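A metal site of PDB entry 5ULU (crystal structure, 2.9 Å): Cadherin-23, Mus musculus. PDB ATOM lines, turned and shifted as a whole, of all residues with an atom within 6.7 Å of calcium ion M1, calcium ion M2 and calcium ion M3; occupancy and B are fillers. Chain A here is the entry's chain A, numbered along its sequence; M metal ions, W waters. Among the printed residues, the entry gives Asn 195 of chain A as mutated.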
ATOM      1  N   GLU A  17      22.195  -0.695  36.897  1.00  0.00           N
ATOM      2  CA  GLU A  17      20.934  -1.393  36.622  1.00  0.00           C
ATOM      3  C   GLU A  17      21.118  -2.900  36.770  1.00  0.00           C
ATOM      4  O   GLU A  17      22.231  -3.426  36.601  1.00  0.00           O
ATOM      5  CB  GLU A  17      20.355  -1.042  35.227  1.00  0.00           C
ATOM      6  CG  GLU A  17      21.269  -1.212  34.025  1.00  0.00           C
ATOM      7  CD  GLU A  17      20.523  -1.360  32.692  1.00  0.00           C
ATOM      8  OE1 GLU A  17      21.149  -1.031  31.649  1.00  0.00           O
ATOM      9  OE2 GLU A  17      19.347  -1.825  32.673  1.00  0.00           O
ATOM     10  N   ASN A  18      20.039  -3.585  37.147  1.00  0.00           N
ATOM     11  CA  ASN A  18      20.035  -5.057  37.326  1.00  0.00           C
ATOM     12  C   ASN A  18      20.734  -5.539  38.590  1.00  0.00           C
ATOM     13  O   ASN A  18      20.679  -6.733  38.863  1.00  0.00           O
ATOM     14  CB  ASN A  18      20.625  -5.810  36.109  1.00  0.00           C
ATOM     15  CG  ASN A  18      19.923  -5.488  34.807  1.00  0.00           C
ATOM     16  OD1 ASN A  18      18.713  -5.606  34.712  1.00  0.00           O
ATOM     17  ND2 ASN A  18      20.693  -5.081  33.779  1.00  0.00           N
ATOM     18  N   ILE A  74      15.721  -3.243  38.548  1.00  0.00           N
ATOM     19  CA  ILE A  74      16.075  -1.864  38.167  1.00  0.00           C
ATOM     20  C   ILE A  74      16.606  -1.790  36.723  1.00  0.00           C
ATOM     21  O   ILE A  74      17.786  -2.038  36.468  1.00  0.00           O
ATOM     22  CB  ILE A  74      17.116  -1.276  39.150  1.00  0.00           C
ATOM     23  CG1 ILE A  74      16.569  -1.305  40.576  1.00  0.00           C
ATOM     24  CG2 ILE A  74      17.487   0.158  38.763  1.00  0.00           C
ATOM     25  CD1 ILE A  74      17.505  -0.689  41.600  1.00  0.00           C
ATOM     26  N   ASP A  75      15.725  -1.397  35.803  1.00  0.00           N
ATOM     27  CA  ASP A  75      16.033  -1.265  34.375  1.00  0.00           C
ATOM     28  C   ASP A  75      16.306   0.210  34.009  1.00  0.00           C
ATOM     29  O   ASP A  75      15.378   1.009  33.972  1.00  0.00           O
ATOM     30  CB  ASP A  75      14.852  -1.818  33.558  1.00  0.00           C
ATOM     31  CG  ASP A  75      15.120  -1.832  32.060  1.00  0.00           C
ATOM     32  OD1 ASP A  75      16.104  -1.257  31.607  1.00  0.00           O
ATOM     33  OD2 ASP A  75      14.336  -2.453  31.334  1.00  0.00           O
ATOM     34  N   ARG A  76      17.560   0.561  33.697  1.00  0.00           N
ATOM     35  CA  ARG A  76      17.890   1.882  33.191  1.00  0.00           C
ATOM     36  C   ARG A  76      17.051   2.247  31.973  1.00  0.00           C
ATOM     37  O   ARG A  76      16.614   3.377  31.835  1.00  0.00           O
ATOM     38  CB  ARG A  76      19.347   1.998  32.793  1.00  0.00           C
ATOM     39  CG  ARG A  76      19.807   3.459  32.744  1.00  0.00           C
ATOM     40  CD  ARG A  76      21.048   3.729  31.903  1.00  0.00           C
ATOM     41  NE  ARG A  76      20.861   3.307  30.523  1.00  0.00           N
ATOM     42  CZ  ARG A  76      20.183   3.982  29.590  1.00  0.00           C
ATOM     43  NH1 ARG A  76      19.588   5.140  29.883  1.00  0.00           N
ATOM     44  NH2 ARG A  76      20.081   3.484  28.364  1.00  0.00           N
ATOM     45  N   GLU A  77      16.810   1.276  31.105  1.00  0.00           N
ATOM     46  CA  GLU A  77      16.036   1.494  29.887  1.00  0.00           C
ATOM     47  C   GLU A  77      14.556   1.885  30.144  1.00  0.00           C
ATOM     48  O   GLU A  77      13.861   2.272  29.237  1.00  0.00           O
ATOM     49  CB  GLU A  77      16.130   0.258  28.977  1.00  0.00           C
ATOM     50  CG  GLU A  77      17.430   0.146  28.177  1.00  0.00           C
ATOM     51  CD  GLU A  77      18.696   0.037  29.016  1.00  0.00           C
ATOM     52  OE1 GLU A  77      19.593   0.882  28.823  1.00  0.00           O
ATOM     53  OE2 GLU A  77      18.831  -0.908  29.853  1.00  0.00           O
ATOM     54  N   ALA A  78      14.098   1.753  31.389  1.00  0.00           N
ATOM     55  CA  ALA A  78      12.739   2.131  31.785  1.00  0.00           C
ATOM     56  C   ALA A  78      12.634   3.483  32.510  1.00  0.00           C
ATOM     57  O   ALA A  78      11.558   3.843  32.940  1.00  0.00           O
ATOM     58  CB  ALA A  78      12.151   1.032  32.663  1.00  0.00           C
ATOM     59  N   LEU A 107      23.326   3.657  36.423  1.00  0.00           N
ATOM     60  CA  LEU A 107      24.321   3.356  35.400  1.00  0.00           C
ATOM     61  C   LEU A 107      23.873   2.261  34.404  1.00  0.00           C
ATOM     62  O   LEU A 107      23.039   1.371  34.751  1.00  0.00           O
ATOM     63  CB  LEU A 107      25.646   2.984  36.047  1.00  0.00           C
ATOM     64  CG  LEU A 107      26.318   4.105  36.843  1.00  0.00           C
ATOM     65  CD1 LEU A 107      27.442   3.515  37.674  1.00  0.00           C
ATOM     66  CD2 LEU A 107      26.821   5.257  35.956  1.00  0.00           C
ATOM     67  N   ASP A 108      24.441   2.331  33.190  1.00  0.00           N
ATOM     68  CA  ASP A 108      24.001   1.509  32.067  1.00  0.00           C
ATOM     69  C   ASP A 108      24.760   0.174  32.003  1.00  0.00           C
ATOM     70  O   ASP A 108      25.987   0.098  32.152  1.00  0.00           O
ATOM     71  CB  ASP A 108      24.162   2.292  30.757  1.00  0.00           C
ATOM     72  CG  ASP A 108      23.641   1.530  29.542  1.00  0.00           C
ATOM     73  OD1 ASP A 108      22.622   0.812  29.655  1.00  0.00           O
ATOM     74  OD2 ASP A 108      24.253   1.694  28.455  1.00  0.00           O
ATOM     75  N   ASP A 109      23.989  -0.870  31.784  1.00  0.00           N
ATOM     76  CA  ASP A 109      24.492  -2.192  31.517  1.00  0.00           C
ATOM     77  C   ASP A 109      24.302  -2.435  30.044  1.00  0.00           C
ATOM     78  O   ASP A 109      23.351  -1.928  29.454  1.00  0.00           O
ATOM     79  CB  ASP A 109      23.660  -3.195  32.308  1.00  0.00           C
ATOM     80  CG  ASP A 109      24.417  -4.414  32.706  1.00  0.00           C
ATOM     81  OD1 ASP A 109      25.657  -4.320  32.739  1.00  0.00           O
ATOM     82  OD2 ASP A 109      23.764  -5.442  33.015  1.00  0.00           O
ATOM     83  N   ASN A 110      25.195  -3.202  29.413  1.00  0.00           N
ATOM     84  CA  ASN A 110      24.956  -3.611  28.026  1.00  0.00           C
ATOM     85  C   ASN A 110      24.071  -4.859  28.023  1.00  0.00           C
ATOM     86  O   ASN A 110      24.546  -5.993  27.843  1.00  0.00           O
ATOM     87  CB  ASN A 110      26.254  -3.822  27.251  1.00  0.00           C
ATOM     88  CG  ASN A 110      26.040  -3.818  25.747  1.00  0.00           C
ATOM     89  OD1 ASN A 110      24.935  -3.506  25.276  1.00  0.00           O
ATOM     90  ND2 ASN A 110      27.079  -4.151  24.988  1.00  0.00           N
ATOM     91  N   ASP A 111      22.766  -4.632  28.212  1.00  0.00           N
ATOM     92  CA  ASP A 111      21.797  -5.732  28.268  1.00  0.00           C
ATOM     93  C   ASP A 111      20.785  -5.713  27.109  1.00  0.00           C
ATOM     94  O   ASP A 111      19.676  -6.275  27.200  1.00  0.00           O
ATOM     95  CB  ASP A 111      21.117  -5.802  29.637  1.00  0.00           C
ATOM     96  CG  ASP A 111      20.541  -4.493  30.091  1.00  0.00           C
ATOM     97  OD1 ASP A 111      20.488  -3.513  29.312  1.00  0.00           O
ATOM     98  OD2 ASP A 111      20.122  -4.459  31.251  1.00  0.00           O
ATOM     99  N   ASN A 112      21.206  -5.121  25.995  1.00  0.00           N
ATOM    100  CA  ASN A 112      20.386  -5.084  24.825  1.00  0.00           C
ATOM    101  C   ASN A 112      21.252  -5.312  23.581  1.00  0.00           C
ATOM    102  O   ASN A 112      22.251  -4.607  23.366  1.00  0.00           O
ATOM    103  CB  ASN A 112      19.607  -3.739  24.742  1.00  0.00           C
ATOM    104  CG  ASN A 112      18.548  -3.603  25.831  1.00  0.00           C
ATOM    105  OD1 ASN A 112      17.495  -4.206  25.741  1.00  0.00           O
ATOM    106  ND2 ASN A 112      18.867  -2.876  26.899  1.00  0.00           N
ATOM    107  N   TRP A 113      20.838  -6.280  22.766  1.00  0.00           N
ATOM    108  CA  TRP A 113      21.617  -6.705  21.618  1.00  0.00           C
ATOM    109  C   TRP A 113      21.324  -5.768  20.457  1.00  0.00           C
ATOM    110  O   TRP A 113      20.180  -5.387  20.252  1.00  0.00           O
ATOM    111  CB  TRP A 113      21.247  -8.115  21.211  1.00  0.00           C
ATOM    112  CG  TRP A 113      21.965  -9.161  21.939  1.00  0.00           C
ATOM    113  CD1 TRP A 113      22.894 -10.039  21.420  1.00  0.00           C
ATOM    114  CD2 TRP A 113      21.823  -9.497  23.308  1.00  0.00           C
ATOM    115  NE1 TRP A 113      23.353 -10.868  22.410  1.00  0.00           N
ATOM    116  CE2 TRP A 113      22.702 -10.566  23.568  1.00  0.00           C
ATOM    117  CE3 TRP A 113      21.050  -8.987  24.348  1.00  0.00           C
ATOM    118  CZ2 TRP A 113      22.819 -11.143  24.820  1.00  0.00           C
ATOM    119  CZ3 TRP A 113      21.175  -9.546  25.589  1.00  0.00           C
ATOM    120  CH2 TRP A 113      22.038 -10.618  25.821  1.00  0.00           C
ATOM    121  N   PRO A 114      22.352  -5.394  19.685  1.00  0.00           N
ATOM    122  CA  PRO A 114      22.077  -4.847  18.355  1.00  0.00           C
ATOM    123  C   PRO A 114      21.042  -5.654  17.573  1.00  0.00           C
ATOM    124  O   PRO A 114      21.224  -6.863  17.349  1.00  0.00           O
ATOM    125  CB  PRO A 114      23.438  -4.917  17.659  1.00  0.00           C
ATOM    126  CG  PRO A 114      24.429  -5.349  18.710  1.00  0.00           C
ATOM    127  CD  PRO A 114      23.767  -5.247  20.041  1.00  0.00           C
ATOM    128  N   ASP A 142      19.734  -0.343  19.097  1.00  0.00           N
ATOM    129  CA  ASP A 142      20.251  -0.820  20.372  1.00  0.00           C
ATOM    130  C   ASP A 142      19.723   0.105  21.464  1.00  0.00           C
ATOM    131  O   ASP A 142      20.042   1.274  21.488  1.00  0.00           O
ATOM    132  CB  ASP A 142      21.795  -0.798  20.336  1.00  0.00           C
ATOM    133  CG  ASP A 142      22.470  -1.489  21.556  1.00  0.00           C
ATOM    134  OD1 ASP A 142      22.194  -1.194  22.747  1.00  0.00           O
ATOM    135  OD2 ASP A 142      23.344  -2.326  21.319  1.00  0.00           O
ATOM    136  N   GLU A 143      18.967  -0.454  22.392  1.00  0.00           N
ATOM    137  CA  GLU A 143      18.316   0.338  23.414  1.00  0.00           C
ATOM    138  C   GLU A 143      19.217   0.836  24.554  1.00  0.00           C
ATOM    139  O   GLU A 143      18.729   1.437  25.499  1.00  0.00           O
ATOM    140  CB  GLU A 143      17.102  -0.430  23.966  1.00  0.00           C
ATOM    141  CG  GLU A 143      16.047  -0.782  22.898  1.00  0.00           C
ATOM    142  CD  GLU A 143      15.394   0.443  22.210  1.00  0.00           C
ATOM    143  OE1 GLU A 143      14.849   1.316  22.915  1.00  0.00           O
ATOM    144  OE2 GLU A 143      15.402   0.504  20.950  1.00  0.00           O
ATOM    145  N   ASP A 144      20.527   0.631  24.490  1.00  0.00           N
ATOM    146  CA  ASP A 144      21.413   1.128  25.556  1.00  0.00           C
ATOM    147  C   ASP A 144      21.938   2.522  25.213  1.00  0.00           C
ATOM    148  O   ASP A 144      21.588   3.100  24.173  1.00  0.00           O
ATOM    149  CB  ASP A 144      22.576   0.148  25.766  1.00  0.00           C
ATOM    150  CG  ASP A 144      22.126  -1.252  26.176  1.00  0.00           C
ATOM    151  OD1 ASP A 144      21.500  -1.402  27.248  1.00  0.00           O
ATOM    152  OD2 ASP A 144      22.463  -2.218  25.440  1.00  0.00           O
ATOM    153  N   SER A 145      22.779   3.048  26.107  1.00  0.00           N
ATOM    154  CA  SER A 145      23.359   4.403  25.984  1.00  0.00           C
ATOM    155  C   SER A 145      24.897   4.351  26.007  1.00  0.00           C
ATOM    156  O   SER A 145      25.497   3.442  26.627  1.00  0.00           O
ATOM    157  CB  SER A 145      22.878   5.267  27.152  1.00  0.00           C
ATOM    158  OG  SER A 145      23.330   4.737  28.396  1.00  0.00           O
ATOM    159  N   LEU A 147      28.775   3.788  24.970  1.00  0.00           N
ATOM    160  CA  LEU A 147      29.500   2.616  24.413  1.00  0.00           C
ATOM    161  C   LEU A 147      28.608   1.418  24.176  1.00  0.00           C
ATOM    162  O   LEU A 147      28.664   0.792  23.113  1.00  0.00           O
ATOM    163  CB  LEU A 147      30.652   2.197  25.350  1.00  0.00           C
ATOM    164  CG  LEU A 147      31.844   3.173  25.376  1.00  0.00           C
ATOM    165  CD1 LEU A 147      32.481   3.253  26.761  1.00  0.00           C
ATOM    166  CD2 LEU A 147      32.857   2.821  24.283  1.00  0.00           C
ATOM    167  N   ASN A 148      27.778   1.115  25.179  1.00  0.00           N
ATOM    168  CA  ASN A 148      26.823  -0.013  25.144  1.00  0.00           C
ATOM    169  C   ASN A 148      25.764   0.081  24.017  1.00  0.00           C
ATOM    170  O   ASN A 148      25.193  -0.938  23.579  1.00  0.00           O
ATOM    171  CB  ASN A 148      26.087  -0.114  26.483  1.00  0.00           C
ATOM    172  CG  ASN A 148      27.003  -0.399  27.637  1.00  0.00           C
ATOM    173  OD1 ASN A 148      28.178  -0.660  27.456  1.00  0.00           O
ATOM    174  ND2 ASN A 148      26.464  -0.352  28.859  1.00  0.00           N
ATOM    175  N   GLY A 149      25.478   1.293  23.577  1.00  0.00           N
ATOM    176  CA  GLY A 149      24.470   1.521  22.567  1.00  0.00           C
ATOM    177  C   GLY A 149      24.966   1.732  21.167  1.00  0.00           C
ATOM    178  O   GLY A 149      24.155   1.745  20.242  1.00  0.00           O
ATOM    179  N   GLU A 150      26.271   1.948  20.987  1.00  0.00           N
ATOM    180  CA  GLU A 150      26.777   2.393  19.667  1.00  0.00           C
ATOM    181  C   GLU A 150      27.173   1.172  18.837  1.00  0.00           C
ATOM    182  O   GLU A 150      27.290   0.078  19.366  1.00  0.00           O
ATOM    183  CB  GLU A 150      27.880   3.480  19.770  1.00  0.00           C
ATOM    184  CG  GLU A 150      29.161   3.116  20.500  1.00  0.00           C
ATOM    185  CD  GLU A 150      30.123   4.294  20.621  1.00  0.00           C
ATOM    186  OE1 GLU A 150      30.437   4.907  19.585  1.00  0.00           O
ATOM    187  OE2 GLU A 150      30.581   4.596  21.759  1.00  0.00           O
ATOM    188  N   ASN A 195      28.452  -3.674  19.496  1.00  0.00           N
ATOM    189  CA  ASN A 195      28.628  -2.647  20.507  1.00  0.00           C
ATOM    190  C   ASN A 195      30.086  -2.528  20.813  1.00  0.00           C
ATOM    191  O   ASN A 195      30.847  -3.473  20.613  1.00  0.00           O
ATOM    192  CB  ASN A 195      27.881  -2.975  21.808  1.00  0.00           C
ATOM    193  CG  ASN A 195      26.370  -2.966  21.655  1.00  0.00           C
ATOM    194  OD1 ASN A 195      25.654  -3.699  22.354  1.00  0.00           O
ATOM    195  ND2 ASN A 195      25.858  -2.102  20.760  1.00  0.00           N
ATOM    196  N   VAL A 199      31.657  -5.480  26.790  1.00  0.00           N
ATOM    197  CA  VAL A 199      30.765  -6.559  26.374  1.00  0.00           C
ATOM    198  C   VAL A 199      30.301  -6.329  24.925  1.00  0.00           C
ATOM    199  O   VAL A 199      29.257  -5.695  24.696  1.00  0.00           O
ATOM    200  CB  VAL A 199      29.556  -6.672  27.339  1.00  0.00           C
ATOM    201  CG1 VAL A 199      28.622  -7.782  26.912  1.00  0.00           C
ATOM    202  CG2 VAL A 199      30.033  -6.918  28.748  1.00  0.00           C
ATOM    203  N   LEU A 201      28.385  -7.098  22.268  1.00  0.00           N
ATOM    204  CA  LEU A 201      27.244  -7.832  21.729  1.00  0.00           C
ATOM    205  C   LEU A 201      27.113  -7.488  20.275  1.00  0.00           C
ATOM    206  O   LEU A 201      27.333  -6.350  19.907  1.00  0.00           O
ATOM    207  CB  LEU A 201      25.945  -7.461  22.419  1.00  0.00           C
ATOM    208  CG  LEU A 201      25.847  -7.610  23.927  1.00  0.00           C
ATOM    209  CD1 LEU A 201      24.418  -7.284  24.373  1.00  0.00           C
ATOM    210  CD2 LEU A 201      26.277  -9.002  24.345  1.00  0.00           C
HETATM  211 CA    CA M   1      23.644  -2.914  23.671  1.00  0.00          CA
HETATM  212 CA    CA M   2      21.230  -1.041  29.536  1.00  0.00          CA
HETATM  213 CA    CA M   3      18.062  -2.830  30.833  1.00  0.00          CA
HETATM  214  O   HOH W   1      17.622  -3.747  32.661  1.00  0.00           O
HETATM  215  O   HOH W   2      17.563  -4.265  28.931  1.00  0.00           O
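Within 4 Å of calcium ion M2: Glu 17, Glu 77, Asp 108, Asp 109, Asp 111, Asn 112 and Asp 144.
Calcium ion M1 is bound by OD1 of Asn 110, O of Asn 112, OD2 of Asp 144, OD1 of Asp 142, OD2 of Asp 142, O of Asn 148 and OD1 of Asn 195.
Water W2 bridges the side-chain amide nitrogen of Asn 112 (2.8 Å) and the backbone carbonyl oxygen of Asp 111 (3.4 Å).
Of the 26 residues printed, 6 come within 4 Å of calcium ion M1.
The nearest printed residue that does not touch calcium ion M1 is Pro 114 (4.3 Å).
Water W1 is bound to calcium ion M3 (2.1 Å).
Calcium ion M3 is bound by the side-chain carboxylate (OE2) of Glu 77, 2.3 Å away.
Calcium ion M3 is bound by water W2 (2.4 Å).
Calcium ion M3 is bound by OE2 of Glu 17, at 2.5 Å.
OD1 of Asp 75 binds calcium ion M3.
The side-chain carboxylate (OD2) of Asp 111 is bound to calcium ion M3 (2.7 Å).
Slightly farther from calcium ion M3 lies OD1 of Asp 111 (2.9 Å).
Calcium ion M2 is bound by the side-chain carboxylate (OE1) of Glu 17 (2.1 Å), the backbone carbonyl oxygen (O) of Asp 109 (2.3 Å), the side-chain carboxylate (OD1) of Asp 108 (2.3 Å), the side-chain carboxylate (OD1) of Asp 144 (2.3 Å), the side-chain carboxylate (OE2) of Glu 77 (2.4 Å), the side-chain carboxylate (OD1) of Asp 111 (2.6 Å) and the side-chain carboxylate (OE1) of Glu 77 (2.6 Å).
Calcium ion M2 has seven donor atoms within binding distance.
Of the 26 residues printed, 4 come within 4 Å of calcium ion M3.
ND2 of Asn 110 lies within hydrogen-bond range of O of Val 199 (2.7 Å).
OD1 of Asp 108 sits close to NE of Arg 76 (3.2 Å).
The backbone NH (N) of Arg 76 sits close to the side-chain carboxylate (OE2) of Glu 17 (3.2 Å).
ND2 of Asn 195 sits at hydrogen-bond distance from O of Glu 150 (3.0 Å).
ND2 of Asn 18 sits close to OD2 of Asp 111, 2.7 Å away.
The side-chain carboxylate (OE1) of Glu 77 lies close to the guanidinium group (NH2) of Arg 76 (2.7 Å).
The backbone NH of Glu 17 sits at hydrogen-bond distance from the backbone carbonyl oxygen of Leu 107, 3.1 Å away.
O of Leu 201 sits at hydrogen-bond distance from N of Asn 195 (2.9 Å).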
